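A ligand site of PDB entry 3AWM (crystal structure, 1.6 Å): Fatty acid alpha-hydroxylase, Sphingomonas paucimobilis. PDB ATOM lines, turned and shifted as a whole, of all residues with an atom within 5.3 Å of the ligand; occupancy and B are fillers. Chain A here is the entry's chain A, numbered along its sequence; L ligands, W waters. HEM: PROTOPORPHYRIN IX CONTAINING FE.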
ATOM      1  N   PHE A  57      16.958  20.202 -26.981  1.00  0.00           N
ATOM      2  CA  PHE A  57      17.077  19.296 -28.154  1.00  0.00           C
ATOM      3  C   PHE A  57      15.717  18.786 -28.626  1.00  0.00           C
ATOM      4  O   PHE A  57      15.488  18.596 -29.831  1.00  0.00           O
ATOM      5  CB  PHE A  57      18.003  18.135 -27.798  1.00  0.00           C
ATOM      6  CG  PHE A  57      18.354  17.258 -28.975  1.00  0.00           C
ATOM      7  CD1 PHE A  57      19.398  17.596 -29.850  1.00  0.00           C
ATOM      8  CD2 PHE A  57      17.666  16.052 -29.183  1.00  0.00           C
ATOM      9  CE1 PHE A  57      19.742  16.767 -30.928  1.00  0.00           C
ATOM     10  CE2 PHE A  57      18.007  15.209 -30.259  1.00  0.00           C
ATOM     11  CZ  PHE A  57      19.049  15.567 -31.142  1.00  0.00           C
ATOM     12  N   TYR A  58      14.817  18.564 -27.667  1.00  0.00           N
ATOM     13  CA  TYR A  58      13.459  18.093 -27.950  1.00  0.00           C
ATOM     14  C   TYR A  58      12.447  19.217 -28.181  1.00  0.00           C
ATOM     15  O   TYR A  58      11.254  18.964 -28.393  1.00  0.00           O
ATOM     16  CB  TYR A  58      12.991  17.110 -26.851  1.00  0.00           C
ATOM     17  CG  TYR A  58      13.683  15.772 -27.059  1.00  0.00           C
ATOM     18  CD1 TYR A  58      13.258  14.892 -28.061  1.00  0.00           C
ATOM     19  CD2 TYR A  58      14.798  15.419 -26.295  1.00  0.00           C
ATOM     20  CE1 TYR A  58      13.914  13.676 -28.267  1.00  0.00           C
ATOM     21  CE2 TYR A  58      15.454  14.212 -26.490  1.00  0.00           C
ATOM     22  CZ  TYR A  58      15.008  13.350 -27.488  1.00  0.00           C
ATOM     23  OH  TYR A  58      15.630  12.139 -27.697  1.00  0.00           O
ATOM     24  N   ARG A  65      14.496  16.980 -37.718  1.00  0.00           N
ATOM     25  CA  ARG A  65      15.250  15.789 -38.076  1.00  0.00           C
ATOM     26  C   ARG A  65      15.398  15.624 -39.562  1.00  0.00           C
ATOM     27  O   ARG A  65      16.270  14.858 -40.002  1.00  0.00           O
ATOM     28  CB  ARG A  65      14.616  14.518 -37.505  1.00  0.00           C
ATOM     29  CG  ARG A  65      14.381  14.586 -35.982  1.00  0.00           C
ATOM     30  CD  ARG A  65      15.653  14.918 -35.185  1.00  0.00           C
ATOM     31  NE  ARG A  65      15.365  14.886 -33.743  1.00  0.00           N
ATOM     32  CZ  ARG A  65      15.387  13.778 -32.987  1.00  0.00           C
ATOM     33  NH1 ARG A  65      15.695  12.597 -33.515  1.00  0.00           N
ATOM     34  NH2 ARG A  65      15.073  13.856 -31.691  1.00  0.00           N
ATOM     35  N   VAL A  83       9.918   6.841 -39.805  1.00  0.00           N
ATOM     36  CA  VAL A  83       9.453   7.879 -38.888  1.00  0.00           C
ATOM     37  C   VAL A  83      10.602   8.765 -38.355  1.00  0.00           C
ATOM     38  O   VAL A  83      10.398   9.953 -38.075  1.00  0.00           O
ATOM     39  CB  VAL A  83       8.645   7.220 -37.726  1.00  0.00           C
ATOM     40  CG1 VAL A  83       9.538   6.304 -36.845  1.00  0.00           C
ATOM     41  CG2 VAL A  83       8.001   8.274 -36.879  1.00  0.00           C
ATOM     42  N   GLN A  84      11.805   8.197 -38.224  1.00  0.00           N
ATOM     43  CA  GLN A  84      12.964   8.962 -37.673  1.00  0.00           C
ATOM     44  C   GLN A  84      13.298  10.201 -38.493  1.00  0.00           C
ATOM     45  O   GLN A  84      13.849  11.167 -37.943  1.00  0.00           O
ATOM     46  CB  GLN A  84      14.208   8.068 -37.586  1.00  0.00           C
ATOM     47  CG  GLN A  84      14.083   6.918 -36.608  1.00  0.00           C
ATOM     48  CD  GLN A  84      13.535   5.638 -37.210  1.00  0.00           C
ATOM     49  OE1 GLN A  84      12.988   5.620 -38.327  1.00  0.00           O
ATOM     50  NE2 GLN A  84      13.671   4.541 -36.458  1.00  0.00           N
ATOM     51  N   HIS A  91       5.264  13.871 -38.934  1.00  0.00           N
ATOM     52  CA  HIS A  91       5.859  13.005 -37.901  1.00  0.00           C
ATOM     53  C   HIS A  91       4.849  12.534 -36.880  1.00  0.00           C
ATOM     54  O   HIS A  91       4.769  11.353 -36.559  1.00  0.00           O
ATOM     55  CB  HIS A  91       7.011  13.700 -37.164  1.00  0.00           C
ATOM     56  CG  HIS A  91       7.482  12.903 -36.002  1.00  0.00           C
ATOM     57  ND1 HIS A  91       7.128  13.207 -34.698  1.00  0.00           N
ATOM     58  CD2 HIS A  91       8.207  11.758 -35.946  1.00  0.00           C
ATOM     59  CE1 HIS A  91       7.622  12.272 -33.900  1.00  0.00           C
ATOM     60  NE2 HIS A  91       8.311  11.398 -34.630  1.00  0.00           N
ATOM     61  N   LYS A  95       3.976   8.765 -35.983  1.00  0.00           N
ATOM     62  CA  LYS A  95       4.382   8.274 -34.659  1.00  0.00           C
ATOM     63  C   LYS A  95       3.190   7.649 -33.899  1.00  0.00           C
ATOM     64  O   LYS A  95       3.351   6.655 -33.198  1.00  0.00           O
ATOM     65  CB  LYS A  95       4.996   9.443 -33.838  1.00  0.00           C
ATOM     66  CG  LYS A  95       5.496   9.079 -32.448  1.00  0.00           C
ATOM     67  CD  LYS A  95       6.477   7.873 -32.470  1.00  0.00           C
ATOM     68  CE  LYS A  95       7.211   7.743 -31.116  1.00  0.00           C
ATOM     69  NZ  LYS A  95       8.186   8.894 -30.935  1.00  0.00           N
ATOM     70  N   PHE A  98       2.881   3.935 -34.399  1.00  0.00           N
ATOM     71  CA  PHE A  98       3.689   3.083 -33.514  1.00  0.00           C
ATOM     72  C   PHE A  98       3.141   3.065 -32.102  1.00  0.00           C
ATOM     73  O   PHE A  98       3.098   2.017 -31.432  1.00  0.00           O
ATOM     74  CB  PHE A  98       5.144   3.573 -33.462  1.00  0.00           C
ATOM     75  CG  PHE A  98       5.921   3.270 -34.724  1.00  0.00           C
ATOM     76  CD1 PHE A  98       6.537   2.036 -34.905  1.00  0.00           C
ATOM     77  CD2 PHE A  98       6.023   4.246 -35.723  1.00  0.00           C
ATOM     78  CE1 PHE A  98       7.240   1.750 -36.087  1.00  0.00           C
ATOM     79  CE2 PHE A  98       6.753   3.974 -36.927  1.00  0.00           C
ATOM     80  CZ  PHE A  98       7.363   2.742 -37.100  1.00  0.00           C
ATOM     81  N   MET A 102       1.272  -0.125 -28.546  1.00  0.00           N
ATOM     82  CA  MET A 102       1.940  -0.350 -27.258  1.00  0.00           C
ATOM     83  C   MET A 102       1.012  -0.409 -26.040  1.00  0.00           C
ATOM     84  O   MET A 102       1.371   0.053 -24.954  1.00  0.00           O
ATOM     85  CB  MET A 102       3.011   0.724 -27.016  1.00  0.00           C
ATOM     86  CG  MET A 102       3.993   0.873 -28.164  1.00  0.00           C
ATOM     87  SD  MET A 102       4.702  -0.742 -28.620  1.00  0.00           S
ATOM     88  CE  MET A 102       5.770  -0.164 -29.944  1.00  0.00           C
ATOM     89  N   ASN A 238      11.228  -1.259 -38.486  1.00  0.00           N
ATOM     90  CA  ASN A 238      11.417  -0.406 -37.298  1.00  0.00           C
ATOM     91  C   ASN A 238      10.738  -0.950 -36.024  1.00  0.00           C
ATOM     92  O   ASN A 238      10.965  -0.388 -34.943  1.00  0.00           O
ATOM     93  CB  ASN A 238      10.942   1.029 -37.564  1.00  0.00           C
ATOM     94  CG  ASN A 238      11.987   1.866 -38.320  1.00  0.00           C
ATOM     95  OD1 ASN A 238      13.193   1.642 -38.210  1.00  0.00           O
ATOM     96  ND2 ASN A 238      11.507   2.832 -39.090  1.00  0.00           N
ATOM     97  N   VAL A 239       9.918  -1.998 -36.147  1.00  0.00           N
ATOM     98  CA  VAL A 239       9.429  -2.766 -34.997  1.00  0.00           C
ATOM     99  C   VAL A 239      10.278  -4.029 -34.793  1.00  0.00           C
ATOM    100  O   VAL A 239      10.742  -4.320 -33.692  1.00  0.00           O
ATOM    101  CB  VAL A 239       7.948  -3.155 -35.206  1.00  0.00           C
ATOM    102  CG1 VAL A 239       7.445  -4.059 -34.053  1.00  0.00           C
ATOM    103  CG2 VAL A 239       7.093  -1.875 -35.314  1.00  0.00           C
ATOM    104  N   PRO A 242      14.554  -3.355 -33.759  1.00  0.00           N
ATOM    105  CA  PRO A 242      14.977  -2.952 -32.406  1.00  0.00           C
ATOM    106  C   PRO A 242      14.516  -3.941 -31.340  1.00  0.00           C
ATOM    107  O   PRO A 242      15.113  -4.010 -30.262  1.00  0.00           O
ATOM    108  CB  PRO A 242      14.334  -1.575 -32.224  1.00  0.00           C
ATOM    109  CG  PRO A 242      13.329  -1.448 -33.282  1.00  0.00           C
ATOM    110  CD  PRO A 242      13.616  -2.403 -34.383  1.00  0.00           C
ATOM    111  N   THR A 243      13.457  -4.703 -31.611  1.00  0.00           N
ATOM    112  CA  THR A 243      13.078  -5.760 -30.656  1.00  0.00           C
ATOM    113  C   THR A 243      14.180  -6.827 -30.568  1.00  0.00           C
ATOM    114  O   THR A 243      14.550  -7.293 -29.466  1.00  0.00           O
ATOM    115  CB  THR A 243      11.710  -6.366 -30.974  1.00  0.00           C
ATOM    116  OG1 THR A 243      10.724  -5.325 -31.026  1.00  0.00           O
ATOM    117  CG2 THR A 243      11.285  -7.377 -29.872  1.00  0.00           C
ATOM    118  N   ALA A 245      17.227  -6.154 -31.123  1.00  0.00           N
ATOM    119  CA  ALA A 245      18.344  -5.460 -30.466  1.00  0.00           C
ATOM    120  C   ALA A 245      18.278  -5.525 -28.938  1.00  0.00           C
ATOM    121  O   ALA A 245      19.281  -5.225 -28.272  1.00  0.00           O
ATOM    122  CB  ALA A 245      18.468  -3.992 -30.981  1.00  0.00           C
ATOM    123  N   ILE A 246      17.138  -5.948 -28.394  1.00  0.00           N
ATOM    124  CA  ILE A 246      17.050  -6.122 -26.931  1.00  0.00           C
ATOM    125  C   ILE A 246      18.046  -7.208 -26.447  1.00  0.00           C
ATOM    126  O   ILE A 246      18.435  -7.199 -25.271  1.00  0.00           O
ATOM    127  CB  ILE A 246      15.594  -6.376 -26.444  1.00  0.00           C
ATOM    128  CG1 ILE A 246      14.663  -5.213 -26.885  1.00  0.00           C
ATOM    129  CG2 ILE A 246      15.512  -6.538 -24.900  1.00  0.00           C
ATOM    130  CD1 ILE A 246      13.181  -5.540 -26.769  1.00  0.00           C
ATOM    131  N   TYR A 249      20.619  -5.510 -24.325  1.00  0.00           N
ATOM    132  CA  TYR A 249      20.264  -5.249 -22.930  1.00  0.00           C
ATOM    133  C   TYR A 249      20.158  -6.521 -22.100  1.00  0.00           C
ATOM    134  O   TYR A 249      20.488  -6.508 -20.907  1.00  0.00           O
ATOM    135  CB  TYR A 249      18.942  -4.500 -22.868  1.00  0.00           C
ATOM    136  CG  TYR A 249      19.030  -2.997 -22.905  1.00  0.00           C
ATOM    137  CD1 TYR A 249      20.034  -2.300 -22.210  1.00  0.00           C
ATOM    138  CD2 TYR A 249      18.031  -2.250 -23.558  1.00  0.00           C
ATOM    139  CE1 TYR A 249      20.089  -0.896 -22.220  1.00  0.00           C
ATOM    140  CE2 TYR A 249      18.065  -0.828 -23.564  1.00  0.00           C
ATOM    141  CZ  TYR A 249      19.095  -0.161 -22.891  1.00  0.00           C
ATOM    142  OH  TYR A 249      19.146   1.215 -22.896  1.00  0.00           O
ATOM    143  N   PHE A 287      24.532   2.002 -24.870  1.00  0.00           N
ATOM    144  CA  PHE A 287      23.838   1.282 -25.942  1.00  0.00           C
ATOM    145  C   PHE A 287      23.622   2.216 -27.134  1.00  0.00           C
ATOM    146  O   PHE A 287      24.305   2.109 -28.134  1.00  0.00           O
ATOM    147  CB  PHE A 287      22.548   0.655 -25.408  1.00  0.00           C
ATOM    148  CG  PHE A 287      21.891  -0.379 -26.330  1.00  0.00           C
ATOM    149  CD1 PHE A 287      22.265  -0.510 -27.668  1.00  0.00           C
ATOM    150  CD2 PHE A 287      20.868  -1.178 -25.845  1.00  0.00           C
ATOM    151  CE1 PHE A 287      21.628  -1.465 -28.491  1.00  0.00           C
ATOM    152  CE2 PHE A 287      20.204  -2.104 -26.646  1.00  0.00           C
ATOM    153  CZ  PHE A 287      20.593  -2.260 -27.991  1.00  0.00           C
ATOM    154  N   PHE A 288      22.643   3.110 -27.019  1.00  0.00           N
ATOM    155  CA  PHE A 288      22.387   4.088 -28.072  1.00  0.00           C
ATOM    156  C   PHE A 288      23.234   5.287 -27.679  1.00  0.00           C
ATOM    157  O   PHE A 288      22.928   5.950 -26.693  1.00  0.00           O
ATOM    158  CB  PHE A 288      20.902   4.476 -28.062  1.00  0.00           C
ATOM    159  CG  PHE A 288      20.333   4.819 -29.424  1.00  0.00           C
ATOM    160  CD1 PHE A 288      20.576   6.056 -29.999  1.00  0.00           C
ATOM    161  CD2 PHE A 288      19.519   3.902 -30.098  1.00  0.00           C
ATOM    162  CE1 PHE A 288      20.022   6.372 -31.247  1.00  0.00           C
ATOM    163  CE2 PHE A 288      18.959   4.220 -31.338  1.00  0.00           C
ATOM    164  CZ  PHE A 288      19.207   5.459 -31.897  1.00  0.00           C
ATOM    165  N   VAL A 291      22.009  11.082 -30.331  1.00  0.00           N
ATOM    166  CA  VAL A 291      20.973  11.395 -31.349  1.00  0.00           C
ATOM    167  C   VAL A 291      21.372  12.649 -32.147  1.00  0.00           C
ATOM    168  O   VAL A 291      22.035  13.539 -31.602  1.00  0.00           O
ATOM    169  CB  VAL A 291      19.607  11.618 -30.664  1.00  0.00           C
ATOM    170  CG1 VAL A 291      18.502  11.944 -31.663  1.00  0.00           C
ATOM    171  CG2 VAL A 291      19.238  10.397 -29.812  1.00  0.00           C
ATOM    172  N   LEU A 316      23.419  10.681 -25.205  1.00  0.00           N
ATOM    173  CA  LEU A 316      22.528   9.978 -24.244  1.00  0.00           C
ATOM    174  C   LEU A 316      23.333   9.344 -23.107  1.00  0.00           C
ATOM    175  O   LEU A 316      22.956   9.484 -21.933  1.00  0.00           O
ATOM    176  CB  LEU A 316      21.697   8.910 -24.967  1.00  0.00           C
ATOM    177  CG  LEU A 316      20.904   9.413 -26.187  1.00  0.00           C
ATOM    178  CD1 LEU A 316      20.131   8.237 -26.804  1.00  0.00           C
ATOM    179  CD2 LEU A 316      19.952  10.570 -25.822  1.00  0.00           C
ATOM    180  N   PRO A 349      18.011   6.868 -21.975  1.00  0.00           N
ATOM    181  CA  PRO A 349      18.666   5.785 -22.724  1.00  0.00           C
ATOM    182  C   PRO A 349      17.999   5.505 -24.088  1.00  0.00           C
ATOM    183  O   PRO A 349      18.659   4.995 -25.001  1.00  0.00           O
ATOM    184  CB  PRO A 349      18.508   4.565 -21.806  1.00  0.00           C
ATOM    185  CG  PRO A 349      17.244   4.871 -21.009  1.00  0.00           C
ATOM    186  CD  PRO A 349      17.331   6.366 -20.755  1.00  0.00           C
ATOM    187  N   GLN A 350      16.710   5.806 -24.197  1.00  0.00           N
ATOM    188  CA  GLN A 350      15.973   5.633 -25.464  1.00  0.00           C
ATOM    189  C   GLN A 350      15.323   6.961 -25.830  1.00  0.00           C
ATOM    190  O   GLN A 350      14.223   7.006 -26.385  1.00  0.00           O
ATOM    191  CB  GLN A 350      14.952   4.471 -25.322  1.00  0.00           C
ATOM    192  CG  GLN A 350      15.683   3.151 -24.919  1.00  0.00           C
ATOM    193  CD  GLN A 350      14.788   1.936 -24.764  1.00  0.00           C
ATOM    194  OE1 GLN A 350      14.896   1.211 -23.761  1.00  0.00           O
ATOM    195  NE2 GLN A 350      13.906   1.697 -25.733  1.00  0.00           N
ATOM    196  N   GLY A 351      16.042   8.050 -25.562  1.00  0.00           N
ATOM    197  CA  GLY A 351      15.554   9.377 -25.914  1.00  0.00           C
ATOM    198  C   GLY A 351      14.806  10.067 -24.781  1.00  0.00           C
ATOM    199  O   GLY A 351      14.474   9.473 -23.752  1.00  0.00           O
ATOM    200  N   GLY A 352      14.527  11.344 -24.987  1.00  0.00           N
ATOM    201  CA  GLY A 352      13.863  12.180 -23.987  1.00  0.00           C
ATOM    202  C   GLY A 352      12.599  12.818 -24.533  1.00  0.00           C
ATOM    203  O   GLY A 352      12.196  12.582 -25.694  1.00  0.00           O
ATOM    204  N   GLY A 358       7.335  14.047 -29.967  1.00  0.00           N
ATOM    205  CA  GLY A 358       8.732  14.067 -30.341  1.00  0.00           C
ATOM    206  C   GLY A 358       9.189  12.688 -30.754  1.00  0.00           C
ATOM    207  O   GLY A 358       8.368  11.774 -30.851  1.00  0.00           O
ATOM    208  N   HIS A 359      10.499  12.536 -30.936  1.00  0.00           N
ATOM    209  CA  HIS A 359      11.051  11.293 -31.484  1.00  0.00           C
ATOM    210  C   HIS A 359      11.413  10.232 -30.439  1.00  0.00           C
ATOM    211  O   HIS A 359      12.031   9.218 -30.775  1.00  0.00           O
ATOM    212  CB  HIS A 359      12.259  11.635 -32.359  1.00  0.00           C
ATOM    213  CG  HIS A 359      11.867  12.245 -33.653  1.00  0.00           C
ATOM    214  ND1 HIS A 359      11.648  11.490 -34.803  1.00  0.00           N
ATOM    215  CD2 HIS A 359      11.618  13.531 -33.996  1.00  0.00           C
ATOM    216  CE1 HIS A 359      11.287  12.300 -35.786  1.00  0.00           C
ATOM    217  NE2 HIS A 359      11.274  13.540 -35.327  1.00  0.00           N
ATOM    218  N   ARG A 360      11.038  10.445 -29.178  1.00  0.00           N
ATOM    219  CA  ARG A 360      11.354   9.471 -28.131  1.00  0.00           C
ATOM    220  C   ARG A 360      10.910   8.060 -28.516  1.00  0.00           C
ATOM    221  O   ARG A 360       9.847   7.848 -29.098  1.00  0.00           O
ATOM    222  CB  ARG A 360      10.658   9.888 -26.809  1.00  0.00           C
ATOM    223  CG  ARG A 360      11.080   9.008 -25.622  1.00  0.00           C
ATOM    224  CD  ARG A 360      10.422   9.561 -24.322  1.00  0.00           C
ATOM    225  NE  ARG A 360      10.883   8.751 -23.204  1.00  0.00           N
ATOM    226  CZ  ARG A 360      11.401   9.246 -22.078  1.00  0.00           C
ATOM    227  NH1 ARG A 360      11.423  10.585 -21.858  1.00  0.00           N
ATOM    228  NH2 ARG A 360      11.867   8.395 -21.155  1.00  0.00           N
ATOM    229  N   CYS A 361      11.732   7.081 -28.153  1.00  0.00           N
ATOM    230  CA  CYS A 361      11.499   5.674 -28.539  1.00  0.00           C
ATOM    231  C   CYS A 361      10.123   5.163 -28.043  1.00  0.00           C
ATOM    232  O   CYS A 361       9.851   5.190 -26.843  1.00  0.00           O
ATOM    233  CB  CYS A 361      12.603   4.831 -27.892  1.00  0.00           C
ATOM    234  SG  CYS A 361      12.403   3.079 -28.269  1.00  0.00           S
ATOM    235  N   PRO A 362       9.284   4.680 -28.958  1.00  0.00           N
ATOM    236  CA  PRO A 362       8.006   4.085 -28.570  1.00  0.00           C
ATOM    237  C   PRO A 362       8.183   2.655 -28.031  1.00  0.00           C
ATOM    238  O   PRO A 362       7.208   2.074 -27.545  1.00  0.00           O
ATOM    239  CB  PRO A 362       7.223   4.054 -29.890  1.00  0.00           C
ATOM    240  CG  PRO A 362       8.304   3.867 -30.964  1.00  0.00           C
ATOM    241  CD  PRO A 362       9.493   4.668 -30.426  1.00  0.00           C
ATOM    242  N   GLY A 363       9.391   2.102 -28.152  1.00  0.00           N
ATOM    243  CA  GLY A 363       9.647   0.742 -27.729  1.00  0.00           C
ATOM    244  C   GLY A 363      10.005   0.579 -26.263  1.00  0.00           C
ATOM    245  O   GLY A 363      10.306  -0.533 -25.835  1.00  0.00           O
ATOM    246  N   ILE A 366       8.041  -2.210 -24.333  1.00  0.00           N
ATOM    247  CA  ILE A 366       8.538  -3.519 -24.760  1.00  0.00           C
ATOM    248  C   ILE A 366       9.899  -3.841 -24.149  1.00  0.00           C
ATOM    249  O   ILE A 366      10.110  -4.950 -23.611  1.00  0.00           O
ATOM    250  CB  ILE A 366       8.626  -3.603 -26.293  1.00  0.00           C
ATOM    251  CG1 ILE A 366       7.193  -3.655 -26.867  1.00  0.00           C
ATOM    252  CG2 ILE A 366       9.452  -4.825 -26.729  1.00  0.00           C
ATOM    253  CD1 ILE A 366       7.106  -3.428 -28.395  1.00  0.00           C
ATOM    254  N   VAL A 367      10.827  -2.896 -24.238  1.00  0.00           N
ATOM    255  CA  VAL A 367      12.171  -3.125 -23.694  1.00  0.00           C
ATOM    256  C   VAL A 367      12.088  -3.463 -22.206  1.00  0.00           C
ATOM    257  O   VAL A 367      12.680  -4.442 -21.752  1.00  0.00           O
ATOM    258  CB  VAL A 367      13.107  -1.914 -23.921  1.00  0.00           C
ATOM    259  CG1 VAL A 367      14.436  -2.101 -23.136  1.00  0.00           C
ATOM    260  CG2 VAL A 367      13.452  -1.807 -25.419  1.00  0.00           C
HETATM  261  CHA HEM L   1      13.634   5.673 -31.549  1.00  0.00           C
HETATM  262  CHB HEM L   1      16.699   3.586 -28.376  1.00  0.00           C
HETATM  263  CHC HEM L   1      14.146  -0.498 -28.680  1.00  0.00           C
HETATM  264  CHD HEM L   1      11.197   1.465 -31.920  1.00  0.00           C
HETATM  265  C1A HEM L   1      14.649   5.456 -30.628  1.00  0.00           C
HETATM  266  C2A HEM L   1      15.620   6.448 -30.232  1.00  0.00           C
HETATM  267  C3A HEM L   1      16.448   5.878 -29.334  1.00  0.00           C
HETATM  268  C4A HEM L   1      16.045   4.510 -29.169  1.00  0.00           C
HETATM  269  CMA HEM L   1      17.652   6.544 -28.638  1.00  0.00           C
HETATM  270  CAA HEM L   1      15.707   7.857 -30.827  1.00  0.00           C
HETATM  271  CBA HEM L   1      15.200   9.013 -29.978  1.00  0.00           C
HETATM  272  CGA HEM L   1      15.264  10.297 -30.780  1.00  0.00           C
HETATM  273  O1A HEM L   1      15.119  11.370 -30.141  1.00  0.00           O
HETATM  274  O2A HEM L   1      15.419  10.278 -32.039  1.00  0.00           O
HETATM  275  C1B HEM L   1      16.345   2.261 -28.302  1.00  0.00           C
HETATM  276  C2B HEM L   1      17.102   1.251 -27.625  1.00  0.00           C
HETATM  277  C3B HEM L   1      16.407   0.101 -27.723  1.00  0.00           C
HETATM  278  C4B HEM L   1      15.168   0.383 -28.461  1.00  0.00           C
HETATM  279  CMB HEM L   1      18.473   1.469 -26.940  1.00  0.00           C
HETATM  280  CAB HEM L   1      16.870  -1.241 -27.175  1.00  0.00           C
HETATM  281  CBB HEM L   1      16.684  -2.414 -27.804  1.00  0.00           C
HETATM  282  C1C HEM L   1      13.025  -0.313 -29.452  1.00  0.00           C
HETATM  283  C2C HEM L   1      11.941  -1.230 -29.685  1.00  0.00           C
HETATM  284  C3C HEM L   1      11.107  -0.706 -30.600  1.00  0.00           C
HETATM  285  C4C HEM L   1      11.668   0.590 -30.960  1.00  0.00           C
HETATM  286  CMC HEM L   1      11.816  -2.586 -28.978  1.00  0.00           C
HETATM  287  CAC HEM L   1       9.804  -1.384 -31.109  1.00  0.00           C
HETATM  288  CBC HEM L   1       8.799  -0.698 -31.656  1.00  0.00           C
HETATM  289  C1D HEM L   1      11.650   2.724 -32.171  1.00  0.00           C
HETATM  290  C2D HEM L   1      11.109   3.597 -33.202  1.00  0.00           C
HETATM  291  C3D HEM L   1      11.838   4.887 -33.064  1.00  0.00           C
HETATM  292  C4D HEM L   1      12.773   4.695 -31.978  1.00  0.00           C
HETATM  293  CMD HEM L   1      10.007   3.293 -34.238  1.00  0.00           C
HETATM  294  CAD HEM L   1      11.658   6.167 -33.892  1.00  0.00           C
HETATM  295  CBD HEM L   1      10.629   7.055 -33.127  1.00  0.00           C
HETATM  296  CGD HEM L   1      10.511   8.431 -33.761  1.00  0.00           C
HETATM  297  O1D HEM L   1       9.525   9.165 -33.484  1.00  0.00           O
HETATM  298  O2D HEM L   1      11.436   8.810 -34.546  1.00  0.00           O
HETATM  299  NA  HEM L   1      14.930   4.258 -29.954  1.00  0.00           N
HETATM  300  NB  HEM L   1      15.164   1.711 -28.802  1.00  0.00           N
HETATM  301  NC  HEM L   1      12.815   0.788 -30.213  1.00  0.00           N
HETATM  302  ND  HEM L   1      12.650   3.402 -31.460  1.00  0.00           N
HETATM  303 FE   HEM L   1      13.847   2.595 -30.046  1.00  0.00          FE
HETATM  304  O   HOH W   1      14.393   8.821 -34.079  1.00  0.00           O
HETATM  305  O   HOH W   2      17.624   9.313 -33.781  1.00  0.00           O
HETATM  306  O   HOH W   3      14.980   1.958 -31.714  1.00  0.00           O
HETATM  307  O   HOH W   4      13.032   1.769 -35.027  1.00  0.00           O
HETATM  308  O   HOH W   5      15.591   4.122 -33.891  1.00  0.00           O
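Water W4 bridges the backbone carbonyl oxygen of Asn 238 and the side-chain amide nitrogen of Gln 84.
The backbone NH (N) of Cys 361 sits at hydrogen-bond distance from the backbone carbonyl oxygen (O) of Gln 350, at 3.1 Å.
The backbone NH of Gly 363 lies close to the side-chain sulfur of Cys 361.
The side-chain hydroxyl (OH) of Tyr 58 lies within hydrogen-bond range of the backbone NH (N) of Gly 352.
A ring nitrogen (ND1) of His 359 sits close to a ring nitrogen (NE2) of His 91 (3.3 Å).
The side-chain amino group of Lys 95 lies within hydrogen-bond range of the backbone carbonyl oxygen of Gly 358.
The side-chain amino group (NZ) of Lys 95 is in hydrogen-bond range of the backbone carbonyl oxygen (O) of Arg 360 (2.7 Å).
The side-chain amide oxygen (OE1) of Gln 84 is in hydrogen-bond range of the side-chain amide nitrogen (ND2) of Asn 238 (3.2 Å).
The side-chain hydroxyl of Thr 243 sits at hydrogen-bond distance from the backbone carbonyl oxygen of Val 239, 2.8 Å away.
SG of Cys 361 binds FE of the ligand (2.3 Å).
An oxygen (O1A) of the ligand sits at hydrogen-bond distance from the side-chain hydroxyl (OH) of Tyr 58 (2.6 Å).
A ring nitrogen (ND1) of His 359 lies within hydrogen-bond range of an oxygen (O2D) of the ligand (2.7 Å).
NH1 of Arg 65 lies within salt-bridge range of O2A of the ligand, 2.8 Å away.
A ring nitrogen (NE2) of His 91 sits at hydrogen-bond distance from an oxygen (O1D) of the ligand, at 2.8 Å.
NZ of Lys 95 lies within salt-bridge range of O1D of the ligand, 2.9 Å away.
NE2 of Gln 350 sits close to NB of the ligand, at 3.3 Å.
Val 83 touches the ligand (CG1 to CAD, 3.6 Å).
Gln 84 touches the ligand (CA to O2D, 3.5 Å).
CE1 of Phe 98 touches CMD of the ligand (3.7 Å).
Met 102 touches the ligand.
Asn 238 touches the ligand.
CA of Val 239 touches CBC of the ligand, at 3.98 Å.
Pro 242 touches the ligand (CB to C1C, 3.3 Å).
Thr 243 touches the ligand.
Ala 245 touches the ligand (C to CBB, 3.7 Å).
Ile 246 touches the ligand.
Tyr 249 touches the ligand (CE2 to CAB, 3.8 Å).
Phe 287 touches the ligand (CE2 to CAB, 3.5 Å).
Phe 288 touches the ligand (CD1 to CMA, 3.3 Å).
Val 291 touches the ligand.
CD1 of Leu 316 touches CMA of the ligand, 3.5 Å away.
N of Gly 351 touches CMA of the ligand, at 3.8 Å.
O of Gly 358 touches O1D of the ligand, at 3.9 Å.
Pro 362 touches the ligand (CD to C2D, 3.4 Å).
CA of Gly 363 touches C3C of the ligand, at 3.5 Å.
Ile 366 touches the ligand (CG2 to CMC, 3.96 Å).
Val 367 touches the ligand (CG2 to CHC, 3.6 Å).
28 residues have an atom within 4 Å of the ligand: Tyr 58, Arg 65, Val 83, Gln 84, His 91, Lys 95, Phe 98, Met 102, Asn 238, Val 239, Pro 242, Thr 243, Ala 245, Ile 246, Tyr 249, Phe 287, Phe 288, Val 291, Leu 316, Gln 350, Gly 351, Gly 358, His 359, Cys 361, Pro 362, Gly 363, Ile 366 and Val 367.
The nearest printed residue that does not touch the ligand is Pro 349 (4.03 Å).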
